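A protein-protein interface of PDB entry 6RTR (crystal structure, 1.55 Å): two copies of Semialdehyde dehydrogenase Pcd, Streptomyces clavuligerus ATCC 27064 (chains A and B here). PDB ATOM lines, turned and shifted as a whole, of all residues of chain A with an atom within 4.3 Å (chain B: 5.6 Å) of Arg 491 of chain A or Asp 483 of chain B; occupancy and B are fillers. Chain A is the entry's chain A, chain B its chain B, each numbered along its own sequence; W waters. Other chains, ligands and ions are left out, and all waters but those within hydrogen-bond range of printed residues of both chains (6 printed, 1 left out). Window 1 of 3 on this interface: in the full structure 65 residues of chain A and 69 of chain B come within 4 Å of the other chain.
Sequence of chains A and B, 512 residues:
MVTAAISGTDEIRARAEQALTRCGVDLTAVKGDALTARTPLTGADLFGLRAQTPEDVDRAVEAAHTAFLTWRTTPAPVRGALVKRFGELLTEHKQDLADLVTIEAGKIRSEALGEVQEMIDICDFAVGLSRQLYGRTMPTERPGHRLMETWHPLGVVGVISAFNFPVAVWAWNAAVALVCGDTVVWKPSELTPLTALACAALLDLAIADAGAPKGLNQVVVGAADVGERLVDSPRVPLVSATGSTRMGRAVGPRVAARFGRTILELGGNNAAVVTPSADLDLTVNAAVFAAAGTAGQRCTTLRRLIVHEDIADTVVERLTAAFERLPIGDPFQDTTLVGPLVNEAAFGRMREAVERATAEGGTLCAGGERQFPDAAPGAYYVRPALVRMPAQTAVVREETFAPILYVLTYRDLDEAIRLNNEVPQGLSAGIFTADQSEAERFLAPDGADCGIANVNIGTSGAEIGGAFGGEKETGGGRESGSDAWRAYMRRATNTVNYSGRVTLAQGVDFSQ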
ATOM      1  N   ARG A 136     -13.548  21.754 -20.610  1.00  0.00           N
ATOM      2  CA  ARG A 136     -12.666  20.608 -20.738  1.00  0.00           C
ATOM      3  C   ARG A 136     -13.475  19.376 -20.922  1.00  0.00           C
ATOM      4  O   ARG A 136     -14.626  19.300 -20.494  1.00  0.00           O
ATOM      5  CB  ARG A 136     -11.793  20.445 -19.488  1.00  0.00           C
ATOM      6  CG  ARG A 136     -10.784  21.577 -19.307  1.00  0.00           C
ATOM      7  CD  ARG A 136      -9.931  21.462 -18.068  1.00  0.00           C
ATOM      8  NE  ARG A 136      -8.671  22.204 -18.227  1.00  0.00           N
ATOM      9  CZ  ARG A 136      -7.808  22.449 -17.239  1.00  0.00           C
ATOM     10  NH1 ARG A 136      -8.067  22.057 -15.992  1.00  0.00           N
ATOM     11  NH2 ARG A 136      -6.680  23.093 -17.497  1.00  0.00           N
ATOM     12  N   GLU A 149     -16.477  19.416 -18.438  1.00  0.00           N
ATOM     13  CA  GLU A 149     -16.735  20.679 -17.769  1.00  0.00           C
ATOM     14  C   GLU A 149     -17.187  21.719 -18.780  1.00  0.00           C
ATOM     15  O   GLU A 149     -16.512  21.919 -19.805  1.00  0.00           O
ATOM     16  CB  GLU A 149     -15.477  21.119 -17.053  1.00  0.00           C
ATOM     17  CG  GLU A 149     -15.491  22.473 -16.423  1.00  0.00           C
ATOM     18  CD  GLU A 149     -14.077  22.860 -16.012  1.00  0.00           C
ATOM     19  OE1 GLU A 149     -13.454  23.708 -16.770  1.00  0.00           O
ATOM     20  OE2 GLU A 149     -13.689  22.290 -14.954  1.00  0.00           O
ATOM     21  N   THR A 150     -18.318  22.347 -18.519  1.00  0.00           N
ATOM     22  CA  THR A 150     -18.952  23.309 -19.441  1.00  0.00           C
ATOM     23  C   THR A 150     -19.104  24.649 -18.739  1.00  0.00           C
ATOM     24  O   THR A 150     -18.975  24.694 -17.519  1.00  0.00           O
ATOM     25  CB  THR A 150     -20.305  22.820 -19.970  1.00  0.00           C
ATOM     26  OG1 THR A 150     -21.144  22.462 -18.858  1.00  0.00           O
ATOM     27  CG2 THR A 150     -20.069  21.586 -20.874  1.00  0.00           C
ATOM     28  N   TRP A 151     -19.155  25.716 -19.521  1.00  0.00           N
ATOM     29  CA  TRP A 151     -19.284  27.066 -18.987  1.00  0.00           C
ATOM     30  C   TRP A 151     -20.554  27.663 -19.519  1.00  0.00           C
ATOM     31  O   TRP A 151     -20.874  27.561 -20.718  1.00  0.00           O
ATOM     32  CB  TRP A 151     -18.043  27.921 -19.349  1.00  0.00           C
ATOM     33  CG  TRP A 151     -16.835  27.510 -18.620  1.00  0.00           C
ATOM     34  CD1 TRP A 151     -15.928  26.545 -19.026  1.00  0.00           C
ATOM     35  CD2 TRP A 151     -16.371  27.963 -17.354  1.00  0.00           C
ATOM     36  NE1 TRP A 151     -14.955  26.378 -18.061  1.00  0.00           N
ATOM     37  CE2 TRP A 151     -15.204  27.257 -17.037  1.00  0.00           C
ATOM     38  CE3 TRP A 151     -16.824  28.929 -16.447  1.00  0.00           C
ATOM     39  CZ2 TRP A 151     -14.500  27.476 -15.869  1.00  0.00           C
ATOM     40  CZ3 TRP A 151     -16.117  29.140 -15.315  1.00  0.00           C
ATOM     41  CH2 TRP A 151     -14.994  28.445 -15.016  1.00  0.00           C
ATOM     42  N   ARG A 486     -13.651  33.811 -17.346  1.00  0.00           N
ATOM     43  CA  ARG A 486     -14.309  32.796 -16.508  1.00  0.00           C
ATOM     44  C   ARG A 486     -15.109  33.386 -15.373  1.00  0.00           C
ATOM     45  O   ARG A 486     -16.060  32.778 -14.888  1.00  0.00           O
ATOM     46  CB  ARG A 486     -13.324  31.833 -15.939  1.00  0.00           C
ATOM     47  CG  ARG A 486     -12.781  30.986 -17.054  1.00  0.00           C
ATOM     48  CD  ARG A 486     -11.957  29.861 -16.526  1.00  0.00           C
ATOM     49  NE  ARG A 486     -11.934  28.757 -17.491  1.00  0.00           N
ATOM     50  CZ  ARG A 486     -11.341  27.593 -17.239  1.00  0.00           C
ATOM     51  NH1 ARG A 486     -10.723  27.379 -16.069  1.00  0.00           N
ATOM     52  NH2 ARG A 486     -11.353  26.643 -18.167  1.00  0.00           N
ATOM     53  N   MET A 489     -18.914  33.741 -16.107  1.00  0.00           N
ATOM     54  CA  MET A 489     -19.677  32.538 -16.410  1.00  0.00           C
ATOM     55  C   MET A 489     -19.699  31.619 -15.195  1.00  0.00           C
ATOM     56  O   MET A 489     -18.949  31.786 -14.228  1.00  0.00           O
ATOM     57  CB  MET A 489     -19.105  31.816 -17.626  1.00  0.00           C
ATOM     58  CG  MET A 489     -19.168  32.664 -18.905  1.00  0.00           C
ATOM     59  SD  MET A 489     -18.647  31.891 -20.417  1.00  0.00           S
ATOM     60  CE  MET A 489     -20.169  31.146 -20.917  1.00  0.00           C
ATOM     61  N   ARG A 490     -20.546  30.586 -15.260  1.00  0.00           N
ATOM     62  CA  ARG A 490     -20.555  29.546 -14.226  1.00  0.00           C
ATOM     63  C   ARG A 490     -20.106  28.200 -14.785  1.00  0.00           C
ATOM     64  O   ARG A 490     -20.500  27.851 -15.887  1.00  0.00           O
ATOM     65  CB  ARG A 490     -21.910  29.389 -13.534  1.00  0.00           C
ATOM     66  CG  ARG A 490     -23.035  29.130 -14.412  1.00  0.00           C
ATOM     67  CD  ARG A 490     -24.314  28.799 -13.580  1.00  0.00           C
ATOM     68  NE  ARG A 490     -25.416  28.754 -14.496  1.00  0.00           N
ATOM     69  CZ  ARG A 490     -25.783  27.721 -15.230  1.00  0.00           C
ATOM     70  NH1 ARG A 490     -25.203  26.538 -15.126  1.00  0.00           N
ATOM     71  NH2 ARG A 490     -26.829  27.865 -16.020  1.00  0.00           N
ATOM     72  N   ARG A 491     -19.289  27.535 -14.002  1.00  0.00           N
ATOM     73  CA  ARG A 491     -18.711  26.226 -14.367  1.00  0.00           C
ATOM     74  C   ARG A 491     -19.736  25.149 -14.035  1.00  0.00           C
ATOM     75  O   ARG A 491     -20.321  25.216 -12.943  1.00  0.00           O
ATOM     76  CB  ARG A 491     -17.460  25.978 -13.541  1.00  0.00           C
ATOM     77  CG  ARG A 491     -16.571  24.822 -13.977  1.00  0.00           C
ATOM     78  CD  ARG A 491     -15.621  24.376 -12.877  1.00  0.00           C
ATOM     79  NE  ARG A 491     -14.719  25.472 -12.474  1.00  0.00           N
ATOM     80  CZ  ARG A 491     -13.399  25.498 -12.667  1.00  0.00           C
ATOM     81  NH1 ARG A 491     -12.758  24.526 -13.332  1.00  0.00           N
ATOM     82  NH2 ARG A 491     -12.703  26.557 -12.221  1.00  0.00           N
ATOM     83  N   ALA A 492     -19.924  24.173 -14.929  1.00  0.00           N
ATOM     84  CA  ALA A 492     -20.709  22.979 -14.587  1.00  0.00           C
ATOM     85  C   ALA A 492     -19.806  21.759 -14.823  1.00  0.00           C
ATOM     86  O   ALA A 492     -19.067  21.714 -15.823  1.00  0.00           O
ATOM     87  CB  ALA A 492     -21.976  22.876 -15.414  1.00  0.00           C
ATOM     88  N   CYS B 450     -27.065  24.039 -11.613  1.00  0.00           N
ATOM     89  CA  CYS B 450     -26.212  23.645 -10.528  1.00  0.00           C
ATOM     90  C   CYS B 450     -24.763  23.533 -10.945  1.00  0.00           C
ATOM     91  O   CYS B 450     -24.426  23.461 -12.124  1.00  0.00           O
ATOM     92  CB  CYS B 450     -26.658  22.283  -9.976  1.00  0.00           C
ATOM     93  SG  CYS B 450     -28.328  22.387  -9.267  1.00  0.00           S
ATOM     94  N   GLY B 451     -23.901  23.383  -9.967  1.00  0.00           N
ATOM     95  CA  GLY B 451     -22.486  23.209 -10.225  1.00  0.00           C
ATOM     96  C   GLY B 451     -22.151  21.853 -10.846  1.00  0.00           C
ATOM     97  O   GLY B 451     -21.138  21.694 -11.534  1.00  0.00           O
ATOM     98  N   ALA B 467     -13.936  19.400 -10.952  1.00  0.00           N
ATOM     99  CA  ALA B 467     -14.080  20.467  -9.985  1.00  0.00           C
ATOM    100  C   ALA B 467     -15.364  20.238  -9.199  1.00  0.00           C
ATOM    101  O   ALA B 467     -16.442  19.934  -9.781  1.00  0.00           O
ATOM    102  CB  ALA B 467     -14.044  21.810 -10.686  1.00  0.00           C
ATOM    103  N   GLU B 471     -23.325  26.435  -6.920  1.00  0.00           N
ATOM    104  CA  GLU B 471     -23.691  27.800  -7.207  1.00  0.00           C
ATOM    105  C   GLU B 471     -24.719  28.310  -6.212  1.00  0.00           C
ATOM    106  O   GLU B 471     -25.182  27.588  -5.298  1.00  0.00           O
ATOM    107  CB  GLU B 471     -24.288  27.828  -8.620  1.00  0.00           C
ATOM    108  CG  GLU B 471     -23.266  27.549  -9.728  1.00  0.00           C
ATOM    109  CD  GLU B 471     -22.099  28.534  -9.668  1.00  0.00           C
ATOM    110  OE1 GLU B 471     -22.363  29.769  -9.699  1.00  0.00           O
ATOM    111  OE2 GLU B 471     -20.913  28.134  -9.535  1.00  0.00           O
ATOM    112  N   ARG B 478     -14.918  25.980  -5.731  1.00  0.00           N
ATOM    113  CA  ARG B 478     -14.619  24.677  -6.299  1.00  0.00           C
ATOM    114  C   ARG B 478     -13.384  24.110  -5.605  1.00  0.00           C
ATOM    115  O   ARG B 478     -12.405  24.837  -5.312  1.00  0.00           O
ATOM    116  CB  ARG B 478     -14.400  24.733  -7.822  1.00  0.00           C
ATOM    117  CG  ARG B 478     -15.615  25.178  -8.646  1.00  0.00           C
ATOM    118  CD  ARG B 478     -16.707  24.109  -8.629  1.00  0.00           C
ATOM    119  NE  ARG B 478     -17.844  24.449  -9.510  1.00  0.00           N
ATOM    120  CZ  ARG B 478     -18.771  25.364  -9.246  1.00  0.00           C
ATOM    121  NH1 ARG B 478     -18.748  26.032  -8.077  1.00  0.00           N
ATOM    122  NH2 ARG B 478     -19.753  25.586 -10.114  1.00  0.00           N
ATOM    123  N   GLY B 481     -10.698  18.730  -8.423  1.00  0.00           N
ATOM    124  CA  GLY B 481     -10.143  18.507  -9.752  1.00  0.00           C
ATOM    125  C   GLY B 481     -10.162  19.679 -10.712  1.00  0.00           C
ATOM    126  O   GLY B 481     -10.337  20.864 -10.313  1.00  0.00           O
ATOM    127  N   SER B 482      -9.988  19.341 -11.998  1.00  0.00           N
ATOM    128  CA  SER B 482      -9.736  20.362 -13.056  1.00  0.00           C
ATOM    129  C   SER B 482      -8.708  21.361 -12.567  1.00  0.00           C
ATOM    130  O   SER B 482      -7.654  20.932 -12.013  1.00  0.00           O
ATOM    131  CB  SER B 482     -11.046  21.010 -13.563  1.00  0.00           C
ATOM    132  OG  SER B 482     -10.868  21.846 -14.727  1.00  0.00           O
ATOM    133  N   ASP B 483      -9.001  22.633 -12.716  1.00  0.00           N
ATOM    134  CA  ASP B 483      -8.078  23.713 -12.246  1.00  0.00           C
ATOM    135  C   ASP B 483      -8.550  24.470 -10.995  1.00  0.00           C
ATOM    136  O   ASP B 483      -8.233  25.636 -10.695  1.00  0.00           O
ATOM    137  CB  ASP B 483      -7.685  24.616 -13.397  1.00  0.00           C
ATOM    138  CG  ASP B 483      -8.838  25.292 -14.007  1.00  0.00           C
ATOM    139  OD1 ASP B 483      -9.970  25.073 -13.512  1.00  0.00           O
ATOM    140  OD2 ASP B 483      -8.586  26.027 -14.983  1.00  0.00           O
ATOM    141  N   ALA B 484      -9.217  23.744 -10.112  1.00  0.00           N
ATOM    142  CA  ALA B 484      -9.529  24.251  -8.788  1.00  0.00           C
ATOM    143  C   ALA B 484      -8.308  24.722  -8.002  1.00  0.00           C
ATOM    144  O   ALA B 484      -8.422  25.622  -7.189  1.00  0.00           O
ATOM    145  CB  ALA B 484     -10.217  23.155  -7.969  1.00  0.00           C
ATOM    146  N   TRP B 485      -7.135  24.126  -8.275  1.00  0.00           N
ATOM    147  CA  TRP B 485      -5.876  24.513  -7.632  1.00  0.00           C
ATOM    148  C   TRP B 485      -5.608  26.030  -7.763  1.00  0.00           C
ATOM    149  O   TRP B 485      -4.927  26.601  -6.921  1.00  0.00           O
ATOM    150  CB  TRP B 485      -4.651  23.764  -8.215  1.00  0.00           C
ATOM    151  CG  TRP B 485      -4.376  23.985  -9.650  1.00  0.00           C
ATOM    152  CD1 TRP B 485      -4.815  23.199 -10.708  1.00  0.00           C
ATOM    153  CD2 TRP B 485      -3.616  25.041 -10.241  1.00  0.00           C
ATOM    154  NE1 TRP B 485      -4.373  23.720 -11.895  1.00  0.00           N
ATOM    155  CE2 TRP B 485      -3.669  24.868 -11.634  1.00  0.00           C
ATOM    156  CE3 TRP B 485      -2.941  26.153  -9.727  1.00  0.00           C
ATOM    157  CZ2 TRP B 485      -3.047  25.754 -12.513  1.00  0.00           C
ATOM    158  CZ3 TRP B 485      -2.325  27.032 -10.612  1.00  0.00           C
ATOM    159  CH2 TRP B 485      -2.366  26.799 -11.981  1.00  0.00           C
ATOM    160  N   ARG B 486      -6.128  26.675  -8.797  1.00  0.00           N
ATOM    161  CA  ARG B 486      -5.845  28.134  -8.958  1.00  0.00           C
ATOM    162  C   ARG B 486      -6.322  28.975  -7.777  1.00  0.00           C
ATOM    163  O   ARG B 486      -5.770  30.017  -7.484  1.00  0.00           O
ATOM    164  CB  ARG B 486      -6.407  28.670 -10.275  1.00  0.00           C
ATOM    165  CG  ARG B 486      -5.730  28.044 -11.480  1.00  0.00           C
ATOM    166  CD  ARG B 486      -6.413  28.457 -12.770  1.00  0.00           C
ATOM    167  NE  ARG B 486      -5.401  28.346 -13.809  1.00  0.00           N
ATOM    168  CZ  ARG B 486      -5.342  29.120 -14.893  1.00  0.00           C
ATOM    169  NH1 ARG B 486      -6.286  30.054 -15.160  1.00  0.00           N
ATOM    170  NH2 ARG B 486      -4.333  28.934 -15.737  1.00  0.00           N
ATOM    171  N   ALA B 487      -7.323  28.517  -7.047  1.00  0.00           N
ATOM    172  CA  ALA B 487      -7.786  29.245  -5.867  1.00  0.00           C
ATOM    173  C   ALA B 487      -6.799  29.239  -4.736  1.00  0.00           C
ATOM    174  O   ALA B 487      -6.902  30.078  -3.823  1.00  0.00           O
ATOM    175  CB  ALA B 487      -9.138  28.672  -5.433  1.00  0.00           C
HETATM  176  O   HOH W   1     -10.068  27.581 -11.134  1.00  0.00           O
HETATM  177  O   HOH W   2     -25.330  23.234 -14.841  1.00  0.00           O
HETATM  178  O   HOH W   3     -14.763  20.127 -13.583  1.00  0.00           O
HETATM  179  O   HOH W   4     -10.879  24.541 -16.499  1.00  0.00           O
HETATM  180  O   HOH W   5     -23.083  25.719 -13.071  1.00  0.00           O
HETATM  181  O   HOH W   6     -18.479  22.689 -11.575  1.00  0.00           O
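The side-chain hydroxyl (OG) of Ser 482 of chain B sits at hydrogen-bond distance from the guanidinium group (NH1) of Arg 136 of chain A (3.1 Å). The side-chain carboxylate (OE2) of Glu 149 of chain A is in hydrogen-bond range of the side-chain hydroxyl (OG) of Ser 482 of chain B (2.9 Å). The guanidinium group of Arg 486 of chain A lies within salt-bridge range of the side-chain carboxylate of Asp 483 of chain B, 2.8 Å away. The backbone carbonyl oxygen (O) of Arg 491 of chain A lies within hydrogen-bond range of the guanidinium group (NH2) of Arg 478 of chain B. NH1 of Arg 491 of chain A is in salt-bridge range of OD1 of Asp 483 of chain B (2.8 Å). NH1 of Arg 136 of chain A sits close to N of Asp 483 of chain B (3.5 Å).
The backbone NH of Glu 149 of chain A is in hydrogen-bond range of the backbone carbonyl oxygen of Arg 136 of chain A (2.8 Å). NE1 of Trp 151 of chain A sits at hydrogen-bond distance from OE1 of Glu 149 of chain A, 3.3 Å away. The side-chain carboxylate of Glu 149 of chain A lies within salt-bridge range of the guanidinium group of Arg 486 of chain A, at 3.9 Å. OE2 of Glu 149 of chain A is in salt-bridge range of NH1 of Arg 491 of chain A (2.9 Å). N of Ala 492 of chain A lies within hydrogen-bond range of O of Thr 150 of chain A, 2.8 Å away. The guanidinium group (NH2) of Arg 478 of chain B lies within salt-bridge range of the side-chain carboxylate (OE2) of Glu 471 of chain B, 2.9 Å away.
Among the printed residues, pairs that only touch across the chains: Arg 490 of chain A with Glu 471 of chain B (3.9 Å), Arg 491 of chain A with Gly 451 of chain B (3.9 Å), Arg 491 of chain A with Ala 467 of chain B (3.7 Å), Arg 491 of chain A with Ser 482 of chain B (3.6 Å) and Ala 492 of chain A with Gly 451 of chain B (3.3 Å).
Arg 491 of chain A touches just these residues of chain B: Gly 451 (3.9 Å), Ala 467 (3.7 Å), Arg 478 (2.9 Å), Ser 482 (3.6 Å) and Asp 483 (2.8 Å). Of the printed residues of chain A, Asp 483 of chain B touches Arg 136, Arg 486 and Arg 491. Of the printed residues of chain B, Arg 486 of chain A touches Asp 483. Of the printed residues of chain A, Gly 451 of chain B touches Arg 491 and Ala 492. Of the printed residues of chain A, Ser 482 of chain B touches Arg 136, Glu 149 and Arg 491. Of the printed residues of chain A, Ala 467 of chain B touches Arg 491. Trp 485 of chain B touches none of the printed residues of chain A. Ala 487 of chain B touches none of the printed residues of chain A. The nearest printed residue of chain A that does not touch Asp 483 of chain B is Glu 149 of chain A (4.9 Å).
Of the 12 printed residues of chain B, 6 touch a printed residue of chain A. Hydrophobic or aromatic side chains of chain B that line the printed part of chain A: Ala 467. Of the 9 printed residues of chain A, 6 touch a printed residue of chain B. Among the printed residues, 11 pairs touch across the chains. Among the printed residues, Asp or Glu carboxylates within 4 Å of a Lys or Arg side-chain nitrogen of the other chain: Arg 486 of chain A with Asp 483 of chain B and Arg 491 of chain A with Asp 483 of chain B.
Position printed for both chains: 486.
Water W1 bridges O of Asp 483 of chain B and NH2 of Arg 491 of chain A. Water W4 lies within hydrogen-bond range of the side-chain carboxylate of Glu 149 of chain A (2.7 Å), the guanidinium group of Arg 486 of chain A (2.7 Å), the side-chain carboxylate of Asp 483 of chain B (3.1 Å) and the side-chain hydroxyl of Ser 482 of chain B (3.2 Å). Water W3 lies within hydrogen-bond range of OE2 of Glu 149 of chain A (2.8 Å) and N of Ala 467 of chain B (2.9 Å). Water W6 lies within hydrogen-bond range of the guanidinium group (NE) of Arg 478 of chain B (2.8 Å), the backbone carbonyl oxygen (O) of Gly 451 of chain B (2.8 Å) and the backbone carbonyl oxygen (O) of Arg 491 of chain A (3.4 Å). Water W5 lies within hydrogen-bond range of the backbone carbonyl oxygen of Cys 450 of chain B (2.8 Å), the backbone carbonyl oxygen of Arg 491 of chain A (2.8 Å) and the guanidinium group of Arg 490 of chain A (3.1 Å). Water W2 bridges O of Cys 450 of chain B (2.9 Å) and NH1 of Arg 490 of chain A (3.3 Å).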
